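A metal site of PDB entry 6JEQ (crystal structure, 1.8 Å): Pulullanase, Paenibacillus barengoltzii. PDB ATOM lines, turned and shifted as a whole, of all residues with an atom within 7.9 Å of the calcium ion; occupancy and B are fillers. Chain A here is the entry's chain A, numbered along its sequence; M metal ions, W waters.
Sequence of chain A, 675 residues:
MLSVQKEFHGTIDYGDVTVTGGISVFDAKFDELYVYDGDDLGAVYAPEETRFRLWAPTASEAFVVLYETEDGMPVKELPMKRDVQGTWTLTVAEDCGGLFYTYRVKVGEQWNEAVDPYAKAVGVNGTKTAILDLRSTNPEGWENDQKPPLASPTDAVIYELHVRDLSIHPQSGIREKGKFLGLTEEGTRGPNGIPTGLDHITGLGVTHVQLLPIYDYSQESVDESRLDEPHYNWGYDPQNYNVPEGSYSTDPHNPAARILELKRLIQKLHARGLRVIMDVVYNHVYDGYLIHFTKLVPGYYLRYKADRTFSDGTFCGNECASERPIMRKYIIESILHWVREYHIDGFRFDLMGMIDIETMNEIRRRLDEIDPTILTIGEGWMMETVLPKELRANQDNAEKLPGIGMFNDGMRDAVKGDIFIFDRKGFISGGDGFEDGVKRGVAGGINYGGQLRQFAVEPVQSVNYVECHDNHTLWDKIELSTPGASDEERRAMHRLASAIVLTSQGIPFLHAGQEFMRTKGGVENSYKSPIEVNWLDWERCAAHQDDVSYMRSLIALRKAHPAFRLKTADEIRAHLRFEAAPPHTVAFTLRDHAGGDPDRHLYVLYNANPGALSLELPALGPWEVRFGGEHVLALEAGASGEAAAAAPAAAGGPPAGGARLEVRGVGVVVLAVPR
OE2 of Glu 224 lies close to N of Gly 246 (3.2 Å).
The backbone NH (N) of Asn 125 sits at hydrogen-bond distance from the side-chain carboxylate (OE1) of Glu 224 (2.9 Å).
The side-chain carboxylate of Glu 224 lies within salt-bridge range of the guanidinium group of Arg 258 (3.3 Å).
The side-chain hydroxyl of Tyr 248 lies within hydrogen-bond range of the side-chain hydroxyl of Tyr 217, at 2.8 Å.
The backbone carbonyl oxygen (O) of Asp 216 sits at hydrogen-bond distance from the backbone NH (N) of Gln 239 (2.9 Å).
The side-chain carboxylate (OD2) of Asp 216 sits at hydrogen-bond distance from the side-chain amide nitrogen (ND2) of Asn 240, at 2.8 Å.
The backbone NH of Asp 216 lies within hydrogen-bond range of the backbone carbonyl oxygen of Val 243 (2.9 Å).
OE2 of Glu 245 is in hydrogen-bond range of OG of Ser 247 (2.6 Å).
Within 4 Å of the calcium ion: Asp 216, Tyr 217, Glu 224 and Glu 245.
Water W3 lies within hydrogen-bond range of OD1 of Asn 125 (2.6 Å), N of Gln 219 (3.3 Å) and O of Val 222 (3.4 Å).
The calcium ion is bound by OE2 of Glu 224 (2.3 Å), water W2 (2.3 Å), O of Tyr 217 (2.3 Å), OD1 of Asp 216 (2.3 Å), OE1 of Glu 245 (2.4 Å), water W1 (2.5 Å) and water W3 (2.5 Å).
The calcium ion has seven donor atoms within binding distance.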
ATOM      1  N   VAL A 122       0.333  -6.824  12.139  1.00  0.00           N
ATOM      2  CA  VAL A 122      -1.026  -6.788  12.686  1.00  0.00           C
ATOM      3  C   VAL A 122      -1.048  -7.458  14.056  1.00  0.00           C
ATOM      4  O   VAL A 122      -0.150  -8.235  14.416  1.00  0.00           O
ATOM      5  CB  VAL A 122      -2.056  -7.477  11.769  1.00  0.00           C
ATOM      6  CG1 VAL A 122      -2.224  -6.727  10.453  1.00  0.00           C
ATOM      7  CG2 VAL A 122      -1.677  -8.961  11.521  1.00  0.00           C
ATOM      8  N   GLY A 123      -2.114  -7.175  14.805  1.00  0.00           N
ATOM      9  CA  GLY A 123      -2.434  -7.918  16.014  1.00  0.00           C
ATOM     10  C   GLY A 123      -3.051  -9.268  15.681  1.00  0.00           C
ATOM     11  O   GLY A 123      -3.248  -9.629  14.524  1.00  0.00           O
ATOM     12  N   VAL A 124      -3.370 -10.035  16.737  1.00  0.00           N
ATOM     13  CA  VAL A 124      -3.897 -11.384  16.529  1.00  0.00           C
ATOM     14  C   VAL A 124      -5.170 -11.307  15.682  1.00  0.00           C
ATOM     15  O   VAL A 124      -5.983 -10.388  15.812  1.00  0.00           O
ATOM     16  CB  VAL A 124      -4.169 -12.096  17.876  1.00  0.00           C
ATOM     17  CG1 VAL A 124      -5.353 -11.471  18.613  1.00  0.00           C
ATOM     18  CG2 VAL A 124      -4.402 -13.592  17.663  1.00  0.00           C
ATOM     19  N   ASN A 125      -5.301 -12.264  14.767  1.00  0.00           N
ATOM     20  CA  ASN A 125      -6.395 -12.359  13.812  1.00  0.00           C
ATOM     21  C   ASN A 125      -6.547 -11.135  12.911  1.00  0.00           C
ATOM     22  O   ASN A 125      -7.578 -10.978  12.256  1.00  0.00           O
ATOM     23  CB  ASN A 125      -7.726 -12.660  14.522  1.00  0.00           C
ATOM     24  CG  ASN A 125      -7.878 -14.144  14.815  1.00  0.00           C
ATOM     25  OD1 ASN A 125      -7.512 -14.985  13.985  1.00  0.00           O
ATOM     26  ND2 ASN A 125      -8.403 -14.468  15.998  1.00  0.00           N
ATOM     27  N   GLY A 126      -5.540 -10.265  12.842  1.00  0.00           N
ATOM     28  CA  GLY A 126      -5.488  -9.247  11.804  1.00  0.00           C
ATOM     29  C   GLY A 126      -6.545  -8.166  11.869  1.00  0.00           C
ATOM     30  O   GLY A 126      -6.918  -7.627  10.823  1.00  0.00           O
ATOM     31  N   TYR A 215       0.705 -15.423   3.403  1.00  0.00           N
ATOM     32  CA  TYR A 215       0.086 -14.151   3.780  1.00  0.00           C
ATOM     33  C   TYR A 215      -1.026 -14.422   4.802  1.00  0.00           C
ATOM     34  O   TYR A 215      -1.436 -15.560   5.042  1.00  0.00           O
ATOM     35  CB  TYR A 215      -0.490 -13.449   2.534  1.00  0.00           C
ATOM     36  CG  TYR A 215      -1.507 -14.315   1.835  1.00  0.00           C
ATOM     37  CD1 TYR A 215      -2.824 -14.409   2.318  1.00  0.00           C
ATOM     38  CD2 TYR A 215      -1.165 -15.085   0.733  1.00  0.00           C
ATOM     39  CE1 TYR A 215      -3.737 -15.237   1.729  1.00  0.00           C
ATOM     40  CE2 TYR A 215      -2.091 -15.908   0.117  1.00  0.00           C
ATOM     41  CZ  TYR A 215      -3.375 -15.985   0.620  1.00  0.00           C
ATOM     42  OH  TYR A 215      -4.300 -16.812   0.037  1.00  0.00           O
ATOM     43  N   ASP A 216      -1.528 -13.339   5.396  1.00  0.00           N
ATOM     44  CA  ASP A 216      -2.499 -13.452   6.481  1.00  0.00           C
ATOM     45  C   ASP A 216      -3.885 -13.749   5.923  1.00  0.00           C
ATOM     46  O   ASP A 216      -4.485 -12.909   5.234  1.00  0.00           O
ATOM     47  CB  ASP A 216      -2.519 -12.172   7.319  1.00  0.00           C
ATOM     48  CG  ASP A 216      -3.406 -12.301   8.551  1.00  0.00           C
ATOM     49  OD1 ASP A 216      -3.586 -13.440   9.000  1.00  0.00           O
ATOM     50  OD2 ASP A 216      -3.917 -11.265   9.063  1.00  0.00           O
ATOM     51  N   TYR A 217      -4.416 -14.925   6.220  1.00  0.00           N
ATOM     52  CA  TYR A 217      -5.743 -15.300   5.756  1.00  0.00           C
ATOM     53  C   TYR A 217      -6.749 -15.277   6.902  1.00  0.00           C
ATOM     54  O   TYR A 217      -6.400 -15.095   8.067  1.00  0.00           O
ATOM     55  CB  TYR A 217      -5.713 -16.651   5.027  1.00  0.00           C
ATOM     56  CG  TYR A 217      -5.078 -17.824   5.739  1.00  0.00           C
ATOM     57  CD1 TYR A 217      -5.799 -18.571   6.668  1.00  0.00           C
ATOM     58  CD2 TYR A 217      -3.784 -18.241   5.420  1.00  0.00           C
ATOM     59  CE1 TYR A 217      -5.247 -19.671   7.286  1.00  0.00           C
ATOM     60  CE2 TYR A 217      -3.227 -19.363   6.032  1.00  0.00           C
ATOM     61  CZ  TYR A 217      -3.965 -20.061   6.977  1.00  0.00           C
ATOM     62  OH  TYR A 217      -3.438 -21.162   7.608  1.00  0.00           O
ATOM     63  N   SER A 218      -8.018 -15.498   6.556  1.00  0.00           N
ATOM     64  CA  SER A 218      -9.120 -15.091   7.410  1.00  0.00           C
ATOM     65  C   SER A 218      -9.227 -15.923   8.687  1.00  0.00           C
ATOM     66  O   SER A 218      -8.828 -17.083   8.750  1.00  0.00           O
ATOM     67  CB  SER A 218     -10.445 -15.188   6.656  1.00  0.00           C
ATOM     68  OG  SER A 218     -10.894 -16.525   6.614  1.00  0.00           O
ATOM     69  N   GLN A 219      -9.818 -15.303   9.704  1.00  0.00           N
ATOM     70  CA  GLN A 219     -10.100 -15.977  10.971  1.00  0.00           C
ATOM     71  C   GLN A 219     -11.085 -17.122  10.782  1.00  0.00           C
ATOM     72  O   GLN A 219     -11.026 -18.121  11.514  1.00  0.00           O
ATOM     73  CB  GLN A 219     -10.636 -14.951  11.973  1.00  0.00           C
ATOM     74  CG  GLN A 219     -11.006 -15.511  13.337  1.00  0.00           C
ATOM     75  CD  GLN A 219     -11.472 -14.411  14.291  1.00  0.00           C
ATOM     76  OE1 GLN A 219     -11.229 -13.229  14.054  1.00  0.00           O
ATOM     77  NE2 GLN A 219     -12.138 -14.808  15.368  1.00  0.00           N
ATOM     78  N   GLU A 220     -12.014 -16.990   9.832  1.00  0.00           N
ATOM     79  CA  GLU A 220     -12.926 -18.092   9.554  1.00  0.00           C
ATOM     80  C   GLU A 220     -12.179 -19.338   9.103  1.00  0.00           C
ATOM     81  O   GLU A 220     -12.638 -20.451   9.327  1.00  0.00           O
ATOM     82  CB  GLU A 220     -13.953 -17.679   8.503  1.00  0.00           C
ATOM     83  CG  GLU A 220     -14.935 -18.774   8.138  1.00  0.00           C
ATOM     84  CD  GLU A 220     -15.622 -19.367   9.367  1.00  0.00           C
ATOM     85  OE1 GLU A 220     -16.196 -18.590  10.148  1.00  0.00           O
ATOM     86  OE2 GLU A 220     -15.573 -20.603   9.534  1.00  0.00           O
ATOM     87  N   SER A 221     -11.027 -19.146   8.459  1.00  0.00           N
ATOM     88  CA  SER A 221     -10.220 -20.280   8.004  1.00  0.00           C
ATOM     89  C   SER A 221      -9.498 -20.930   9.181  1.00  0.00           C
ATOM     90  O   SER A 221      -9.619 -22.144   9.406  1.00  0.00           O
ATOM     91  CB  SER A 221      -9.199 -19.819   6.968  1.00  0.00           C
ATOM     92  OG  SER A 221      -9.814 -19.039   5.971  1.00  0.00           O
ATOM     93  N   VAL A 222      -8.722 -20.142   9.904  1.00  0.00           N
ATOM     94  CA  VAL A 222      -8.001 -20.587  11.100  1.00  0.00           C
ATOM     95  C   VAL A 222      -8.100 -19.454  12.117  1.00  0.00           C
ATOM     96  O   VAL A 222      -7.678 -18.331  11.823  1.00  0.00           O
ATOM     97  CB  VAL A 222      -6.532 -20.931  10.814  1.00  0.00           C
ATOM     98  CG1 VAL A 222      -5.796 -21.170  12.124  1.00  0.00           C
ATOM     99  CG2 VAL A 222      -6.430 -22.156   9.907  1.00  0.00           C
ATOM    100  N   ASP A 223      -8.650 -19.747  13.284  1.00  0.00           N
ATOM    101  CA  ASP A 223      -8.758 -18.755  14.354  1.00  0.00           C
ATOM    102  C   ASP A 223      -7.454 -18.727  15.143  1.00  0.00           C
ATOM    103  O   ASP A 223      -7.147 -19.674  15.878  1.00  0.00           O
ATOM    104  CB  ASP A 223      -9.946 -19.079  15.259  1.00  0.00           C
ATOM    105  CG  ASP A 223     -10.231 -17.978  16.255  1.00  0.00           C
ATOM    106  OD1 ASP A 223      -9.282 -17.250  16.651  1.00  0.00           O
ATOM    107  OD2 ASP A 223     -11.402 -17.841  16.662  1.00  0.00           O
ATOM    108  N   GLU A 224      -6.699 -17.631  15.012  1.00  0.00           N
ATOM    109  CA  GLU A 224      -5.374 -17.507  15.600  1.00  0.00           C
ATOM    110  C   GLU A 224      -5.398 -17.410  17.118  1.00  0.00           C
ATOM    111  O   GLU A 224      -4.344 -17.542  17.742  1.00  0.00           O
ATOM    112  CB  GLU A 224      -4.637 -16.286  15.041  1.00  0.00           C
ATOM    113  CG  GLU A 224      -4.330 -16.370  13.546  1.00  0.00           C
ATOM    114  CD  GLU A 224      -3.770 -15.069  13.035  1.00  0.00           C
ATOM    115  OE1 GLU A 224      -3.374 -14.243  13.873  1.00  0.00           O
ATOM    116  OE2 GLU A 224      -3.708 -14.882  11.800  1.00  0.00           O
ATOM    117  N   ASP A 237      -8.056 -17.563   1.509  1.00  0.00           N
ATOM    118  CA  ASP A 237      -9.031 -16.560   1.941  1.00  0.00           C
ATOM    119  C   ASP A 237      -8.295 -15.326   2.421  1.00  0.00           C
ATOM    120  O   ASP A 237      -8.171 -15.090   3.633  1.00  0.00           O
ATOM    121  CB  ASP A 237      -9.929 -17.123   3.058  1.00  0.00           C
ATOM    122  CG  ASP A 237     -10.493 -18.496   2.717  1.00  0.00           C
ATOM    123  OD1 ASP A 237     -11.232 -18.582   1.726  1.00  0.00           O
ATOM    124  OD2 ASP A 237     -10.204 -19.490   3.432  1.00  0.00           O
ATOM    125  N   GLN A 239      -6.847 -11.920   3.818  1.00  0.00           N
ATOM    126  CA  GLN A 239      -7.305 -10.821   4.665  1.00  0.00           C
ATOM    127  C   GLN A 239      -6.315  -9.669   4.681  1.00  0.00           C
ATOM    128  O   GLN A 239      -6.708  -8.537   4.383  1.00  0.00           O
ATOM    129  CB  GLN A 239      -7.573 -11.315   6.088  1.00  0.00           C
ATOM    130  CG  GLN A 239      -8.388 -10.337   6.888  1.00  0.00           C
ATOM    131  CD  GLN A 239      -8.583 -10.756   8.318  1.00  0.00           C
ATOM    132  OE1 GLN A 239      -8.661 -11.940   8.627  1.00  0.00           O
ATOM    133  NE2 GLN A 239      -8.646  -9.767   9.215  1.00  0.00           N
ATOM    134  N   ASN A 240      -5.046  -9.906   5.039  1.00  0.00           N
ATOM    135  CA  ASN A 240      -4.014  -8.870   4.994  1.00  0.00           C
ATOM    136  C   ASN A 240      -2.890  -9.347   4.071  1.00  0.00           C
ATOM    137  O   ASN A 240      -2.106 -10.241   4.439  1.00  0.00           O
ATOM    138  CB  ASN A 240      -3.500  -8.539   6.390  1.00  0.00           C
ATOM    139  CG  ASN A 240      -4.592  -7.974   7.286  1.00  0.00           C
ATOM    140  OD1 ASN A 240      -5.100  -6.873   7.043  1.00  0.00           O
ATOM    141  ND2 ASN A 240      -4.965  -8.728   8.315  1.00  0.00           N
ATOM    142  N   VAL A 243       1.269  -9.017   5.253  1.00  0.00           N
ATOM    143  CA  VAL A 243       1.776  -9.500   6.544  1.00  0.00           C
ATOM    144  C   VAL A 243       1.661 -11.021   6.538  1.00  0.00           C
ATOM    145  O   VAL A 243       0.772 -11.566   5.853  1.00  0.00           O
ATOM    146  CB  VAL A 243       0.976  -8.852   7.697  1.00  0.00           C
ATOM    147  CG1 VAL A 243      -0.452  -9.187   7.576  1.00  0.00           C
ATOM    148  CG2 VAL A 243       1.500  -9.262   9.081  1.00  0.00           C
ATOM    149  N   PRO A 244       2.521 -11.760   7.242  1.00  0.00           N
ATOM    150  CA  PRO A 244       2.407 -13.219   7.256  1.00  0.00           C
ATOM    151  C   PRO A 244       1.215 -13.696   8.073  1.00  0.00           C
ATOM    152  O   PRO A 244       0.617 -12.971   8.881  1.00  0.00           O
ATOM    153  CB  PRO A 244       3.716 -13.674   7.914  1.00  0.00           C
ATOM    154  CG  PRO A 244       4.655 -12.558   7.724  1.00  0.00           C
ATOM    155  CD  PRO A 244       3.795 -11.320   7.835  1.00  0.00           C
ATOM    156  N   GLU A 245       0.879 -14.967   7.867  1.00  0.00           N
ATOM    157  CA  GLU A 245      -0.208 -15.624   8.602  1.00  0.00           C
ATOM    158  C   GLU A 245       0.194 -15.873  10.051  1.00  0.00           C
ATOM    159  O   GLU A 245       1.286 -16.392  10.335  1.00  0.00           O
ATOM    160  CB  GLU A 245      -0.595 -16.926   7.917  1.00  0.00           C
ATOM    161  CG  GLU A 245      -1.331 -17.944   8.790  1.00  0.00           C
ATOM    162  CD  GLU A 245      -2.671 -17.457   9.314  1.00  0.00           C
ATOM    163  OE1 GLU A 245      -3.251 -16.492   8.760  1.00  0.00           O
ATOM    164  OE2 GLU A 245      -3.195 -18.067  10.274  1.00  0.00           O
ATOM    165  N   GLY A 246      -0.693 -15.500  10.981  1.00  0.00           N
ATOM    166  CA  GLY A 246      -0.333 -15.570  12.388  1.00  0.00           C
ATOM    167  C   GLY A 246      -0.232 -16.982  12.923  1.00  0.00           C
ATOM    168  O   GLY A 246       0.566 -17.245  13.832  1.00  0.00           O
ATOM    169  N   SER A 247      -1.019 -17.922  12.388  1.00  0.00           N
ATOM    170  CA  SER A 247      -1.021 -19.260  12.943  1.00  0.00           C
ATOM    171  C   SER A 247       0.255 -20.035  12.637  1.00  0.00           C
ATOM    172  O   SER A 247       0.489 -21.079  13.259  1.00  0.00           O
ATOM    173  CB  SER A 247      -2.230 -20.064  12.444  1.00  0.00           C
ATOM    174  OG  SER A 247      -2.129 -20.344  11.051  1.00  0.00           O
ATOM    175  N   TYR A 248       1.098 -19.552  11.719  1.00  0.00           N
ATOM    176  CA  TYR A 248       2.381 -20.185  11.477  1.00  0.00           C
ATOM    177  C   TYR A 248       3.493 -19.602  12.347  1.00  0.00           C
ATOM    178  O   TYR A 248       4.653 -19.974  12.172  1.00  0.00           O
ATOM    179  CB  TYR A 248       2.764 -20.073   9.983  1.00  0.00           C
ATOM    180  CG  TYR A 248       1.730 -20.666   9.048  1.00  0.00           C
ATOM    181  CD1 TYR A 248       0.952 -21.765   9.441  1.00  0.00           C
ATOM    182  CD2 TYR A 248       1.526 -20.149   7.774  1.00  0.00           C
ATOM    183  CE1 TYR A 248      -0.015 -22.302   8.604  1.00  0.00           C
ATOM    184  CE2 TYR A 248       0.559 -20.706   6.923  1.00  0.00           C
ATOM    185  CZ  TYR A 248      -0.191 -21.780   7.339  1.00  0.00           C
ATOM    186  OH  TYR A 248      -1.162 -22.320   6.527  1.00  0.00           O
ATOM    187  N   ARG A 258       5.797 -13.369  13.872  1.00  0.00           N
ATOM    188  CA  ARG A 258       5.545 -13.979  12.570  1.00  0.00           C
ATOM    189  C   ARG A 258       6.468 -13.415  11.486  1.00  0.00           C
ATOM    190  O   ARG A 258       6.854 -14.137  10.562  1.00  0.00           O
ATOM    191  CB  ARG A 258       4.085 -13.787  12.180  1.00  0.00           C
ATOM    192  CG  ARG A 258       3.697 -12.316  11.907  1.00  0.00           C
ATOM    193  CD  ARG A 258       2.221 -12.173  11.575  1.00  0.00           C
ATOM    194  NE  ARG A 258       1.392 -12.265  12.781  1.00  0.00           N
ATOM    195  CZ  ARG A 258       0.060 -12.280  12.749  1.00  0.00           C
ATOM    196  NH1 ARG A 258      -0.578 -12.221  11.589  1.00  0.00           N
ATOM    197  NH2 ARG A 258      -0.638 -12.371  13.899  1.00  0.00           N
HETATM  198 CA    CA M   1      -4.938 -15.131   9.892  1.00  0.00          CA
HETATM  199  O   HOH W   1      -6.090 -12.889  10.110  1.00  0.00           O
HETATM  200  O   HOH W   2      -5.675 -17.326  10.135  1.00  0.00           O
HETATM  201  O   HOH W   3      -6.960 -14.982  11.419  1.00  0.00           O
